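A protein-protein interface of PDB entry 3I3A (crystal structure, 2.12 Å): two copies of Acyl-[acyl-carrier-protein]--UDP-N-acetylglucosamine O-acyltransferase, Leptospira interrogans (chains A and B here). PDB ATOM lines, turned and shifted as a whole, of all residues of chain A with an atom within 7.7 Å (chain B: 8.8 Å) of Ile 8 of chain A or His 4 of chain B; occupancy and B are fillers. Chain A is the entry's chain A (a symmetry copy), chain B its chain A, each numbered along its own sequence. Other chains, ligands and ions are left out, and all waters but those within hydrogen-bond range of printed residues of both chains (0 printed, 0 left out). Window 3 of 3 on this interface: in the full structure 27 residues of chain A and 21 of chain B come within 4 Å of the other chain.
OG1 of Thr 6 of chain A lies within hydrogen-bond range of N of Tyr 24 of chain A, 3.1 Å away. The backbone carbonyl oxygen (O) of Pro 23 of chain B sits at hydrogen-bond distance from the backbone NH (N) of His 42 of chain B (2.9 Å). The backbone NH (N) of Tyr 24 of chain B lies within hydrogen-bond range of the side-chain hydroxyl (OG1) of Thr 6 of chain B (3.1 Å). N of Ile 27 of chain A lies within hydrogen-bond range of O of Ile 8 of chain A (2.8 Å). N of His 4 of chain B sits at hydrogen-bond distance from O of Val 21 of chain B, 2.8 Å away. N of Ile 8 of chain A sits at hydrogen-bond distance from O of Ser 25 of chain A (2.8 Å).
Ile 8 of chain A touches just these residues of chain B: His 4, Pro 23 and Tyr 24. Of chain A, only Ile 8 (3.8 Å) comes within 4 Å of His 4 of chain B. No residue of chain B comes within 4 Å of Ala 7 of chain A. Of the printed residues of chain A, Pro 23 of chain B touches Ile 8 (3.7 Å). Printed residues of chain B within 4 Å of Tyr 24 of chain A: Tyr 24 and His 42. Printed residues of chain A within 4 Å of Tyr 24 of chain B: Thr 6, Ile 8 and Tyr 24. Of the printed residues of chain B, Ile 26 of chain A touches His 42 (3.9 Å). Printed residues of chain A within 4 Å of His 42 of chain B: Tyr 24 (3.1 Å) and Ile 26 (3.9 Å). Ile 9 of chain B touches none of the printed residues of chain A. Val 21 of chain A touches none of the printed residues of chain B. The nearest residue of chain B that does not touch Ile 8 of chain A is Thr 6 of chain B (5.0 Å). The nearest printed residue of chain A that does not touch His 42 of chain B is Val 43 of chain A (5.1 Å).
Among the printed residues, pairs that only touch across the chains: Tyr 24 of chain A with Tyr 24 of chain B (3.2 Å), Ile 8 of chain A with Tyr 24 of chain B (3.6 Å), Ile 8 of chain A with Pro 23 of chain B (3.7 Å), Ile 8 of chain A with His 4 of chain B (3.8 Å) and Ile 26 of chain A with His 42 of chain B (3.9 Å).
Thr 6 of chain A touches Tyr 24 of chain B, but with the chains exchanged Tyr 24 of chain A does not touch Thr 6 of chain B (6.6 Å). Ile 8 of chain A touches His 4 of chain B, but with the chains exchanged His 4 of chain A does not touch Ile 8 of chain B (14.0 Å). Ile 8 of chain A touches Pro 23 of chain B, but with the chains exchanged Pro 23 of chain A does not touch Ile 8 of chain B (13.1 Å). Ile 8 of chain A touches Tyr 24 of chain B, but with the chains exchanged Tyr 24 of chain A does not touch Ile 8 of chain B (8.6 Å). 12 positions are printed for both chains. Of the 7 pairs that touch across the chains among the printed residues, 1 has its exchanged pair printed and touching as well.
The side-chain hydroxyl (OH) of Tyr 24 of chain B lies within hydrogen-bond range of the backbone carbonyl oxygen (O) of Thr 6 of chain A (2.4 Å). A ring nitrogen (NE2) of His 42 of chain B lies within hydrogen-bond range of the backbone carbonyl oxygen of Tyr 24 of chain A (3.1 Å).
Of the 20 printed residues of chain B, 4 touch a printed residue of chain A. Printed residues of chain B that touch a printed residue of chain A: His 4, Pro 23, Tyr 24 and His 42. Hydrophobic or aromatic side chains of chain B that line the printed part of chain A: His 4, Pro 23, Tyr 24 and His 42. Printed residues of chain A that touch a printed residue of chain B: Thr 6, Ile 8, Tyr 24 and Ile 26. Among the printed residues, no Asp or Glu carboxylate lies within 4 Å of a Lys or Arg side-chain nitrogen of the other chain.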
ATOM      1  N   ILE A   3      36.231   3.686  13.869  1.00  0.00           N
ATOM      2  CA  ILE A   3      35.591   4.948  14.224  1.00  0.00           C
ATOM      3  C   ILE A   3      34.107   4.679  14.455  1.00  0.00           C
ATOM      4  O   ILE A   3      33.444   4.105  13.583  1.00  0.00           O
ATOM      5  CB  ILE A   3      35.753   5.988  13.084  1.00  0.00           C
ATOM      6  CG1 ILE A   3      37.228   6.381  12.919  1.00  0.00           C
ATOM      7  CG2 ILE A   3      34.864   7.208  13.339  1.00  0.00           C
ATOM      8  CD1 ILE A   3      37.593   6.937  11.550  1.00  0.00           C
ATOM      9  N   HIS A   4      33.588   5.086  15.616  1.00  0.00           N
ATOM     10  CA  HIS A   4      32.202   4.781  15.980  1.00  0.00           C
ATOM     11  C   HIS A   4      31.153   5.460  15.080  1.00  0.00           C
ATOM     12  O   HIS A   4      31.268   6.651  14.790  1.00  0.00           O
ATOM     13  CB  HIS A   4      31.916   5.096  17.452  1.00  0.00           C
ATOM     14  CG  HIS A   4      30.642   4.483  17.950  1.00  0.00           C
ATOM     15  ND1 HIS A   4      29.446   5.167  17.975  1.00  0.00           N
ATOM     16  CD2 HIS A   4      30.371   3.234  18.400  1.00  0.00           C
ATOM     17  CE1 HIS A   4      28.497   4.374  18.438  1.00  0.00           C
ATOM     18  NE2 HIS A   4      29.032   3.194  18.703  1.00  0.00           N
ATOM     19  N   PRO A   5      30.133   4.689  14.634  1.00  0.00           N
ATOM     20  CA  PRO A   5      29.011   5.155  13.796  1.00  0.00           C
ATOM     21  C   PRO A   5      28.470   6.549  14.127  1.00  0.00           C
ATOM     22  O   PRO A   5      28.213   7.334  13.213  1.00  0.00           O
ATOM     23  CB  PRO A   5      27.920   4.102  14.062  1.00  0.00           C
ATOM     24  CG  PRO A   5      28.675   2.853  14.324  1.00  0.00           C
ATOM     25  CD  PRO A   5      30.035   3.239  14.896  1.00  0.00           C
ATOM     26  N   THR A   6      28.310   6.845  15.415  1.00  0.00           N
ATOM     27  CA  THR A   6      27.717   8.112  15.861  1.00  0.00           C
ATOM     28  C   THR A   6      28.713   9.272  16.001  1.00  0.00           C
ATOM     29  O   THR A   6      28.315  10.407  16.268  1.00  0.00           O
ATOM     30  CB  THR A   6      26.959   7.947  17.202  1.00  0.00           C
ATOM     31  OG1 THR A   6      27.883   7.649  18.261  1.00  0.00           O
ATOM     32  CG2 THR A   6      25.899   6.848  17.104  1.00  0.00           C
ATOM     33  N   ALA A   7      30.000   8.988  15.841  1.00  0.00           N
ATOM     34  CA  ALA A   7      31.019  10.032  15.907  1.00  0.00           C
ATOM     35  C   ALA A   7      30.848  10.981  14.726  1.00  0.00           C
ATOM     36  O   ALA A   7      30.608  10.546  13.590  1.00  0.00           O
ATOM     37  CB  ALA A   7      32.404   9.425  15.901  1.00  0.00           C
ATOM     38  N   ILE A   8      30.955  12.278  15.005  1.00  0.00           N
ATOM     39  CA  ILE A   8      30.815  13.300  13.974  1.00  0.00           C
ATOM     40  C   ILE A   8      32.195  13.844  13.587  1.00  0.00           C
ATOM     41  O   ILE A   8      32.804  14.627  14.320  1.00  0.00           O
ATOM     42  CB  ILE A   8      29.823  14.416  14.407  1.00  0.00           C
ATOM     43  CG1 ILE A   8      28.464  13.789  14.784  1.00  0.00           C
ATOM     44  CG2 ILE A   8      29.662  15.457  13.297  1.00  0.00           C
ATOM     45  CD1 ILE A   8      27.550  14.677  15.611  1.00  0.00           C
ATOM     46  N   ILE A   9      32.694  13.393  12.438  1.00  0.00           N
ATOM     47  CA  ILE A   9      34.012  13.822  11.957  1.00  0.00           C
ATOM     48  C   ILE A   9      33.903  14.563  10.627  1.00  0.00           C
ATOM     49  O   ILE A   9      33.375  14.033   9.638  1.00  0.00           O
ATOM     50  CB  ILE A   9      35.015  12.646  11.833  1.00  0.00           C
ATOM     51  CG1 ILE A   9      35.151  11.900  13.167  1.00  0.00           C
ATOM     52  CG2 ILE A   9      36.381  13.149  11.357  1.00  0.00           C
ATOM     53  CD1 ILE A   9      35.822  10.570  13.060  1.00  0.00           C
ATOM     54  N   ASP A  10      34.405  15.795  10.623  1.00  0.00           N
ATOM     55  CA  ASP A  10      34.474  16.603   9.415  1.00  0.00           C
ATOM     56  C   ASP A  10      35.249  15.830   8.353  1.00  0.00           C
ATOM     57  O   ASP A  10      36.288  15.240   8.667  1.00  0.00           O
ATOM     58  CB  ASP A  10      35.155  17.938   9.729  1.00  0.00           C
ATOM     59  CG  ASP A  10      35.158  18.896   8.551  1.00  0.00           C
ATOM     60  OD1 ASP A  10      35.821  18.596   7.541  1.00  0.00           O
ATOM     61  OD2 ASP A  10      34.520  19.962   8.641  1.00  0.00           O
ATOM     62  N   PRO A  11      34.738  15.812   7.096  1.00  0.00           N
ATOM     63  CA  PRO A  11      35.400  15.157   5.958  1.00  0.00           C
ATOM     64  C   PRO A  11      36.845  15.606   5.692  1.00  0.00           C
ATOM     65  O   PRO A  11      37.634  14.830   5.152  1.00  0.00           O
ATOM     66  CB  PRO A  11      34.505  15.538   4.762  1.00  0.00           C
ATOM     67  CG  PRO A  11      33.654  16.672   5.234  1.00  0.00           C
ATOM     68  CD  PRO A  11      33.451  16.410   6.691  1.00  0.00           C
ATOM     69  N   ALA A  13      39.088  16.590   8.081  1.00  0.00           N
ATOM     70  CA  ALA A  13      39.997  16.109   9.118  1.00  0.00           C
ATOM     71  C   ALA A  13      40.852  14.952   8.580  1.00  0.00           C
ATOM     72  O   ALA A  13      40.334  14.050   7.915  1.00  0.00           O
ATOM     73  CB  ALA A  13      39.215  15.683  10.359  1.00  0.00           C
ATOM     74  N   VAL A  21      38.040   6.314  17.229  1.00  0.00           N
ATOM     75  CA  VAL A  21      37.210   7.412  17.726  1.00  0.00           C
ATOM     76  C   VAL A  21      35.951   6.800  18.306  1.00  0.00           C
ATOM     77  O   VAL A  21      35.249   6.055  17.616  1.00  0.00           O
ATOM     78  CB  VAL A  21      36.829   8.431  16.607  1.00  0.00           C
ATOM     79  CG1 VAL A  21      36.083   9.628  17.200  1.00  0.00           C
ATOM     80  CG2 VAL A  21      38.056   8.910  15.866  1.00  0.00           C
ATOM     81  N   GLY A  22      35.676   7.094  19.574  1.00  0.00           N
ATOM     82  CA  GLY A  22      34.554   6.473  20.261  1.00  0.00           C
ATOM     83  C   GLY A  22      33.240   7.208  20.059  1.00  0.00           C
ATOM     84  O   GLY A  22      33.193   8.207  19.333  1.00  0.00           O
ATOM     85  N   PRO A  23      32.164   6.714  20.705  1.00  0.00           N
ATOM     86  CA  PRO A  23      30.791   7.204  20.586  1.00  0.00           C
ATOM     87  C   PRO A  23      30.595   8.686  20.875  1.00  0.00           C
ATOM     88  O   PRO A  23      31.046   9.186  21.915  1.00  0.00           O
ATOM     89  CB  PRO A  23      30.036   6.389  21.640  1.00  0.00           C
ATOM     90  CG  PRO A  23      30.836   5.161  21.828  1.00  0.00           C
ATOM     91  CD  PRO A  23      32.255   5.561  21.625  1.00  0.00           C
ATOM     92  N   TYR A  24      29.906   9.367  19.953  1.00  0.00           N
ATOM     93  CA  TYR A  24      29.430  10.751  20.142  1.00  0.00           C
ATOM     94  C   TYR A  24      30.559  11.794  20.294  1.00  0.00           C
ATOM     95  O   TYR A  24      30.347  12.863  20.866  1.00  0.00           O
ATOM     96  CB  TYR A  24      28.405  10.846  21.308  1.00  0.00           C
ATOM     97  CG  TYR A  24      27.310   9.792  21.278  1.00  0.00           C
ATOM     98  CD1 TYR A  24      27.198   8.835  22.290  1.00  0.00           C
ATOM     99  CD2 TYR A  24      26.406   9.731  20.216  1.00  0.00           C
ATOM    100  CE1 TYR A  24      26.196   7.854  22.253  1.00  0.00           C
ATOM    101  CE2 TYR A  24      25.401   8.758  20.164  1.00  0.00           C
ATOM    102  CZ  TYR A  24      25.300   7.820  21.180  1.00  0.00           C
ATOM    103  OH  TYR A  24      24.299   6.866  21.107  1.00  0.00           O
ATOM    104  N   SER A  25      31.744  11.467  19.779  1.00  0.00           N
ATOM    105  CA  SER A  25      32.873  12.401  19.729  1.00  0.00           C
ATOM    106  C   SER A  25      32.800  13.260  18.471  1.00  0.00           C
ATOM    107  O   SER A  25      32.275  12.821  17.440  1.00  0.00           O
ATOM    108  CB  SER A  25      34.203  11.649  19.749  1.00  0.00           C
ATOM    109  OG  SER A  25      34.403  11.007  20.987  1.00  0.00           O
ATOM    110  N   ILE A  26      33.348  14.469  18.554  1.00  0.00           N
ATOM    111  CA  ILE A  26      33.209  15.467  17.506  1.00  0.00           C
ATOM    112  C   ILE A  26      34.572  15.958  17.058  1.00  0.00           C
ATOM    113  O   ILE A  26      35.323  16.559  17.845  1.00  0.00           O
ATOM    114  CB  ILE A  26      32.358  16.669  17.989  1.00  0.00           C
ATOM    115  CG1 ILE A  26      31.012  16.178  18.532  1.00  0.00           C
ATOM    116  CG2 ILE A  26      32.176  17.711  16.869  1.00  0.00           C
ATOM    117  CD1 ILE A  26      30.260  17.191  19.355  1.00  0.00           C
ATOM    118  N   ILE A  27      34.901  15.700  15.796  1.00  0.00           N
ATOM    119  CA  ILE A  27      36.178  16.152  15.246  1.00  0.00           C
ATOM    120  C   ILE A  27      35.928  17.139  14.108  1.00  0.00           C
ATOM    121  O   ILE A  27      35.224  16.829  13.135  1.00  0.00           O
ATOM    122  CB  ILE A  27      37.087  14.978  14.793  1.00  0.00           C
ATOM    123  CG1 ILE A  27      37.224  13.937  15.920  1.00  0.00           C
ATOM    124  CG2 ILE A  27      38.466  15.505  14.350  1.00  0.00           C
ATOM    125  CD1 ILE A  27      38.039  12.705  15.561  1.00  0.00           C
ATOM    126  N   GLU A  28      36.494  18.336  14.252  1.00  0.00           N
ATOM    127  CA  GLU A  28      36.219  19.420  13.311  1.00  0.00           C
ATOM    128  C   GLU A  28      37.184  19.387  12.133  1.00  0.00           C
ATOM    129  O   GLU A  28      38.068  18.524  12.069  1.00  0.00           O
ATOM    130  CB  GLU A  28      36.266  20.780  14.020  1.00  0.00           C
ATOM    131  CG  GLU A  28      35.351  20.869  15.233  1.00  0.00           C
ATOM    132  CD  GLU A  28      35.187  22.278  15.771  1.00  0.00           C
ATOM    133  OE1 GLU A  28      36.123  23.088  15.656  1.00  0.00           O
ATOM    134  OE2 GLU A  28      34.110  22.570  16.326  1.00  0.00           O
ATOM    135  N   VAL A  43      34.361  13.086  23.201  1.00  0.00           N
ATOM    136  CA  VAL A  43      35.580  13.888  23.082  1.00  0.00           C
ATOM    137  C   VAL A  43      35.372  14.920  21.977  1.00  0.00           C
ATOM    138  O   VAL A  43      34.727  14.629  20.972  1.00  0.00           O
ATOM    139  CB  VAL A  43      36.823  13.012  22.777  1.00  0.00           C
ATOM    140  CG1 VAL A  43      38.051  13.869  22.451  1.00  0.00           C
ATOM    141  CG2 VAL A  43      37.110  12.061  23.942  1.00  0.00           C
ATOM    142  N   ILE A  45      37.522  17.491  19.415  1.00  0.00           N
ATOM    143  CA  ILE A  45      38.773  17.946  18.817  1.00  0.00           C
ATOM    144  C   ILE A  45      38.470  19.104  17.861  1.00  0.00           C
ATOM    145  O   ILE A  45      37.817  18.921  16.827  1.00  0.00           O
ATOM    146  CB  ILE A  45      39.524  16.808  18.061  1.00  0.00           C
ATOM    147  CG1 ILE A  45      39.648  15.525  18.914  1.00  0.00           C
ATOM    148  CG2 ILE A  45      40.875  17.304  17.548  1.00  0.00           C
ATOM    149  CD1 ILE A  45      40.622  15.604  20.117  1.00  0.00           C
ATOM    150  N   MET B   1      18.006  29.715  11.698  1.00  0.00           N
ATOM    151  CA  MET B   1      19.263  29.002  12.084  1.00  0.00           C
ATOM    152  C   MET B   1      19.011  27.510  12.360  1.00  0.00           C
ATOM    153  O   MET B   1      17.896  27.021  12.147  1.00  0.00           O
ATOM    154  CB  MET B   1      19.931  29.693  13.271  1.00  0.00           C
ATOM    155  N   LYS B   2      20.033  26.792  12.833  1.00  0.00           N
ATOM    156  CA  LYS B   2      20.025  25.323  12.766  1.00  0.00           C
ATOM    157  C   LYS B   2      20.197  24.574  14.092  1.00  0.00           C
ATOM    158  O   LYS B   2      21.121  24.833  14.867  1.00  0.00           O
ATOM    159  CB  LYS B   2      21.030  24.832  11.707  1.00  0.00           C
ATOM    160  CG  LYS B   2      21.065  23.327  11.530  1.00  0.00           C
ATOM    161  CD  LYS B   2      21.074  22.935  10.061  1.00  0.00           C
ATOM    162  CE  LYS B   2      20.567  21.515   9.887  1.00  0.00           C
ATOM    163  NZ  LYS B   2      20.288  21.207   8.461  1.00  0.00           N
ATOM    164  N   ILE B   3      19.283  23.629  14.312  1.00  0.00           N
ATOM    165  CA  ILE B   3      19.287  22.726  15.456  1.00  0.00           C
ATOM    166  C   ILE B   3      19.732  21.349  14.971  1.00  0.00           C
ATOM    167  O   ILE B   3      19.150  20.815  14.020  1.00  0.00           O
ATOM    168  CB  ILE B   3      17.870  22.618  16.078  1.00  0.00           C
ATOM    169  CG1 ILE B   3      17.450  23.959  16.696  1.00  0.00           C
ATOM    170  CG2 ILE B   3      17.815  21.479  17.098  1.00  0.00           C
ATOM    171  CD1 ILE B   3      15.946  24.155  16.840  1.00  0.00           C
ATOM    172  N   HIS B   4      20.752  20.777  15.616  1.00  0.00           N
ATOM    173  CA  HIS B   4      21.324  19.507  15.163  1.00  0.00           C
ATOM    174  C   HIS B   4      20.362  18.310  15.275  1.00  0.00           C
ATOM    175  O   HIS B   4      19.705  18.141  16.303  1.00  0.00           O
ATOM    176  CB  HIS B   4      22.644  19.190  15.872  1.00  0.00           C
ATOM    177  CG  HIS B   4      23.428  18.103  15.202  1.00  0.00           C
ATOM    178  ND1 HIS B   4      23.354  16.782  15.589  1.00  0.00           N
ATOM    179  CD2 HIS B   4      24.269  18.136  14.140  1.00  0.00           C
ATOM    180  CE1 HIS B   4      24.130  16.052  14.810  1.00  0.00           C
ATOM    181  NE2 HIS B   4      24.697  16.850  13.921  1.00  0.00           N
ATOM    182  N   PRO B   5      20.278  17.484  14.205  1.00  0.00           N
ATOM    183  CA  PRO B   5      19.449  16.266  14.126  1.00  0.00           C
ATOM    184  C   PRO B   5      19.379  15.427  15.406  1.00  0.00           C
ATOM    185  O   PRO B   5      18.295  14.976  15.778  1.00  0.00           O
ATOM    186  CB  PRO B   5      20.133  15.452  13.014  1.00  0.00           C
ATOM    187  CG  PRO B   5      20.699  16.479  12.105  1.00  0.00           C
ATOM    188  CD  PRO B   5      20.988  17.727  12.933  1.00  0.00           C
ATOM    189  N   THR B   6      20.520  15.232  16.065  1.00  0.00           N
ATOM    190  CA  THR B   6      20.603  14.376  17.253  1.00  0.00           C
ATOM    191  C   THR B   6      20.277  15.081  18.578  1.00  0.00           C
ATOM    192  O   THR B   6      20.214  14.440  19.628  1.00  0.00           O
ATOM    193  CB  THR B   6      21.994  13.706  17.379  1.00  0.00           C
ATOM    194  OG1 THR B   6      22.999  14.699  17.643  1.00  0.00           O
ATOM    195  CG2 THR B   6      22.346  12.924  16.112  1.00  0.00           C
ATOM    196  N   ALA B   7      20.091  16.394  18.534  1.00  0.00           N
ATOM    197  CA  ALA B   7      19.730  17.148  19.732  1.00  0.00           C
ATOM    198  C   ALA B   7      18.334  16.736  20.187  1.00  0.00           C
ATOM    199  O   ALA B   7      17.419  16.577  19.365  1.00  0.00           O
ATOM    200  CB  ALA B   7      19.781  18.636  19.461  1.00  0.00           C
ATOM    201  N   ILE B   8      18.184  16.550  21.494  1.00  0.00           N
ATOM    202  CA  ILE B   8      16.904  16.154  22.073  1.00  0.00           C
ATOM    203  C   ILE B   8      16.235  17.364  22.738  1.00  0.00           C
ATOM    204  O   ILE B   8      16.626  17.794  23.826  1.00  0.00           O
ATOM    205  CB  ILE B   8      17.060  14.943  23.034  1.00  0.00           C
ATOM    206  CG1 ILE B   8      17.742  13.774  22.294  1.00  0.00           C
ATOM    207  CG2 ILE B   8      15.701  14.522  23.599  1.00  0.00           C
ATOM    208  CD1 ILE B   8      18.335  12.699  23.189  1.00  0.00           C
ATOM    209  N   ILE B   9      15.242  17.926  22.053  1.00  0.00           N
ATOM    210  CA  ILE B   9      14.527  19.099  22.568  1.00  0.00           C
ATOM    211  C   ILE B   9      13.050  18.793  22.795  1.00  0.00           C
ATOM    212  O   ILE B   9      12.330  18.378  21.874  1.00  0.00           O
ATOM    213  CB  ILE B   9      14.681  20.343  21.654  1.00  0.00           C
ATOM    214  CG1 ILE B   9      16.161  20.676  21.429  1.00  0.00           C
ATOM    215  CG2 ILE B   9      13.943  21.545  22.249  1.00  0.00           C
ATOM    216  CD1 ILE B   9      16.410  21.633  20.309  1.00  0.00           C
ATOM    217  N   VAL B  19      17.887  30.484  17.260  1.00  0.00           N
ATOM    218  CA  VAL B  19      18.653  29.650  18.199  1.00  0.00           C
ATOM    219  C   VAL B  19      19.285  28.415  17.535  1.00  0.00           C
ATOM    220  O   VAL B  19      18.615  27.655  16.813  1.00  0.00           O
ATOM    221  CB  VAL B  19      17.813  29.231  19.457  1.00  0.00           C
ATOM    222  CG1 VAL B  19      18.623  28.327  20.403  1.00  0.00           C
ATOM    223  CG2 VAL B  19      17.324  30.448  20.212  1.00  0.00           C
ATOM    224  N   GLU B  20      20.586  28.255  17.778  1.00  0.00           N
ATOM    225  CA  GLU B  20      21.355  27.108  17.316  1.00  0.00           C
ATOM    226  C   GLU B  20      21.630  26.158  18.468  1.00  0.00           C
ATOM    227  O   GLU B  20      21.964  26.597  19.570  1.00  0.00           O
ATOM    228  CB  GLU B  20      22.672  27.570  16.706  1.00  0.00           C
ATOM    229  CG  GLU B  20      22.494  28.266  15.376  1.00  0.00           C
ATOM    230  CD  GLU B  20      23.696  29.085  14.973  1.00  0.00           C
ATOM    231  OE1 GLU B  20      24.833  28.687  15.297  1.00  0.00           O
ATOM    232  OE2 GLU B  20      23.496  30.136  14.333  1.00  0.00           O
ATOM    233  N   VAL B  21      21.466  24.864  18.207  1.00  0.00           N
ATOM    234  CA  VAL B  21      21.673  23.815  19.208  1.00  0.00           C
ATOM    235  C   VAL B  21      22.533  22.744  18.568  1.00  0.00           C
ATOM    236  O   VAL B  21      22.181  22.217  17.509  1.00  0.00           O
ATOM    237  CB  VAL B  21      20.334  23.185  19.702  1.00  0.00           C
ATOM    238  CG1 VAL B  21      20.592  22.199  20.843  1.00  0.00           C
ATOM    239  CG2 VAL B  21      19.367  24.252  20.160  1.00  0.00           C
ATOM    240  N   GLY B  22      23.667  22.438  19.194  1.00  0.00           N
ATOM    241  CA  GLY B  22      24.618  21.505  18.610  1.00  0.00           C
ATOM    242  C   GLY B  22      24.323  20.053  18.946  1.00  0.00           C
ATOM    243  O   GLY B  22      23.329  19.762  19.621  1.00  0.00           O
ATOM    244  N   PRO B  23      25.191  19.134  18.475  1.00  0.00           N
ATOM    245  CA  PRO B  23      25.057  17.683  18.600  1.00  0.00           C
ATOM    246  C   PRO B  23      24.887  17.159  20.019  1.00  0.00           C
ATOM    247  O   PRO B  23      25.672  17.507  20.913  1.00  0.00           O
ATOM    248  CB  PRO B  23      26.380  17.160  18.033  1.00  0.00           C
ATOM    249  CG  PRO B  23      26.864  18.225  17.129  1.00  0.00           C
ATOM    250  CD  PRO B  23      26.411  19.509  17.730  1.00  0.00           C
ATOM    251  N   TYR B  24      23.869  16.312  20.202  1.00  0.00           N
ATOM    252  CA  TYR B  24      23.662  15.535  21.440  1.00  0.00           C
ATOM    253  C   TYR B  24      23.372  16.397  22.688  1.00  0.00           C
ATOM    254  O   TYR B  24      23.599  15.959  23.815  1.00  0.00           O
ATOM    255  CB  TYR B  24      24.833  14.542  21.692  1.00  0.00           C
ATOM    256  CG  TYR B  24      25.239  13.718  20.480  1.00  0.00           C
ATOM    257  CD1 TYR B  24      26.504  13.851  19.904  1.00  0.00           C
ATOM    258  CD2 TYR B  24      24.340  12.829  19.889  1.00  0.00           C
ATOM    259  CE1 TYR B  24      26.871  13.101  18.778  1.00  0.00           C
ATOM    260  CE2 TYR B  24      24.691  12.073  18.764  1.00  0.00           C
ATOM    261  CZ  TYR B  24      25.954  12.213  18.209  1.00  0.00           C
ATOM    262  OH  TYR B  24      26.278  11.456  17.096  1.00  0.00           O
ATOM    263  N   SER B  25      22.873  17.613  22.467  1.00  0.00           N
ATOM    264  CA  SER B  25      22.426  18.496  23.550  1.00  0.00           C
ATOM    265  C   SER B  25      20.976  18.199  23.916  1.00  0.00           C
ATOM    266  O   SER B  25      20.189  17.765  23.066  1.00  0.00           O
ATOM    267  CB  SER B  25      22.552  19.964  23.141  1.00  0.00           C
ATOM    268  OG  SER B  25      23.903  20.334  22.994  1.00  0.00           O
ATOM    269  N   ILE B  39      23.917  27.238  21.370  1.00  0.00           N
ATOM    270  CA  ILE B  39      24.183  26.101  22.241  1.00  0.00           C
ATOM    271  C   ILE B  39      25.010  25.089  21.460  1.00  0.00           C
ATOM    272  O   ILE B  39      24.590  24.650  20.383  1.00  0.00           O
ATOM    273  CB  ILE B  39      22.850  25.457  22.719  1.00  0.00           C
ATOM    274  CG1 ILE B  39      22.127  26.398  23.693  1.00  0.00           C
ATOM    275  CG2 ILE B  39      23.102  24.125  23.386  1.00  0.00           C
ATOM    276  CD1 ILE B  39      20.614  26.332  23.653  1.00  0.00           C
ATOM    277  N   GLU B  40      26.173  24.707  21.991  1.00  0.00           N
ATOM    278  CA  GLU B  40      27.043  23.739  21.284  1.00  0.00           C
ATOM    279  C   GLU B  40      26.692  22.328  21.785  1.00  0.00           C
ATOM    280  O   GLU B  40      25.764  22.169  22.585  1.00  0.00           O
ATOM    281  CB  GLU B  40      28.529  23.931  21.668  1.00  0.00           C
ATOM    282  CG  GLU B  40      29.147  25.228  21.149  1.00  0.00           C
ATOM    283  CD  GLU B  40      30.597  25.436  21.569  1.00  0.00           C
ATOM    284  OE1 GLU B  40      31.196  24.531  22.204  1.00  0.00           O
ATOM    285  OE2 GLU B  40      31.141  26.519  21.262  1.00  0.00           O
ATOM    286  N   GLY B  41      27.414  21.314  21.312  1.00  0.00           N
ATOM    287  CA  GLY B  41      27.166  19.935  21.731  1.00  0.00           C
ATOM    288  C   GLY B  41      27.228  19.518  23.188  1.00  0.00           C
ATOM    289  O   GLY B  41      27.894  20.167  23.985  1.00  0.00           O
ATOM    290  N   HIS B  42      26.516  18.444  23.529  1.00  0.00           N
ATOM    291  CA  HIS B  42      26.495  17.849  24.882  1.00  0.00           C
ATOM    292  C   HIS B  42      26.092  18.826  25.991  1.00  0.00           C
ATOM    293  O   HIS B  42      26.441  18.634  27.161  1.00  0.00           O
ATOM    294  CB  HIS B  42      27.851  17.215  25.246  1.00  0.00           C
ATOM    295  CG  HIS B  42      28.349  16.228  24.238  1.00  0.00           C
ATOM    296  ND1 HIS B  42      29.581  16.343  23.636  1.00  0.00           N
ATOM    297  CD2 HIS B  42      27.782  15.112  23.723  1.00  0.00           C
ATOM    298  CE1 HIS B  42      29.752  15.344  22.790  1.00  0.00           C
ATOM    299  NE2 HIS B  42      28.675  14.580  22.825  1.00  0.00           N
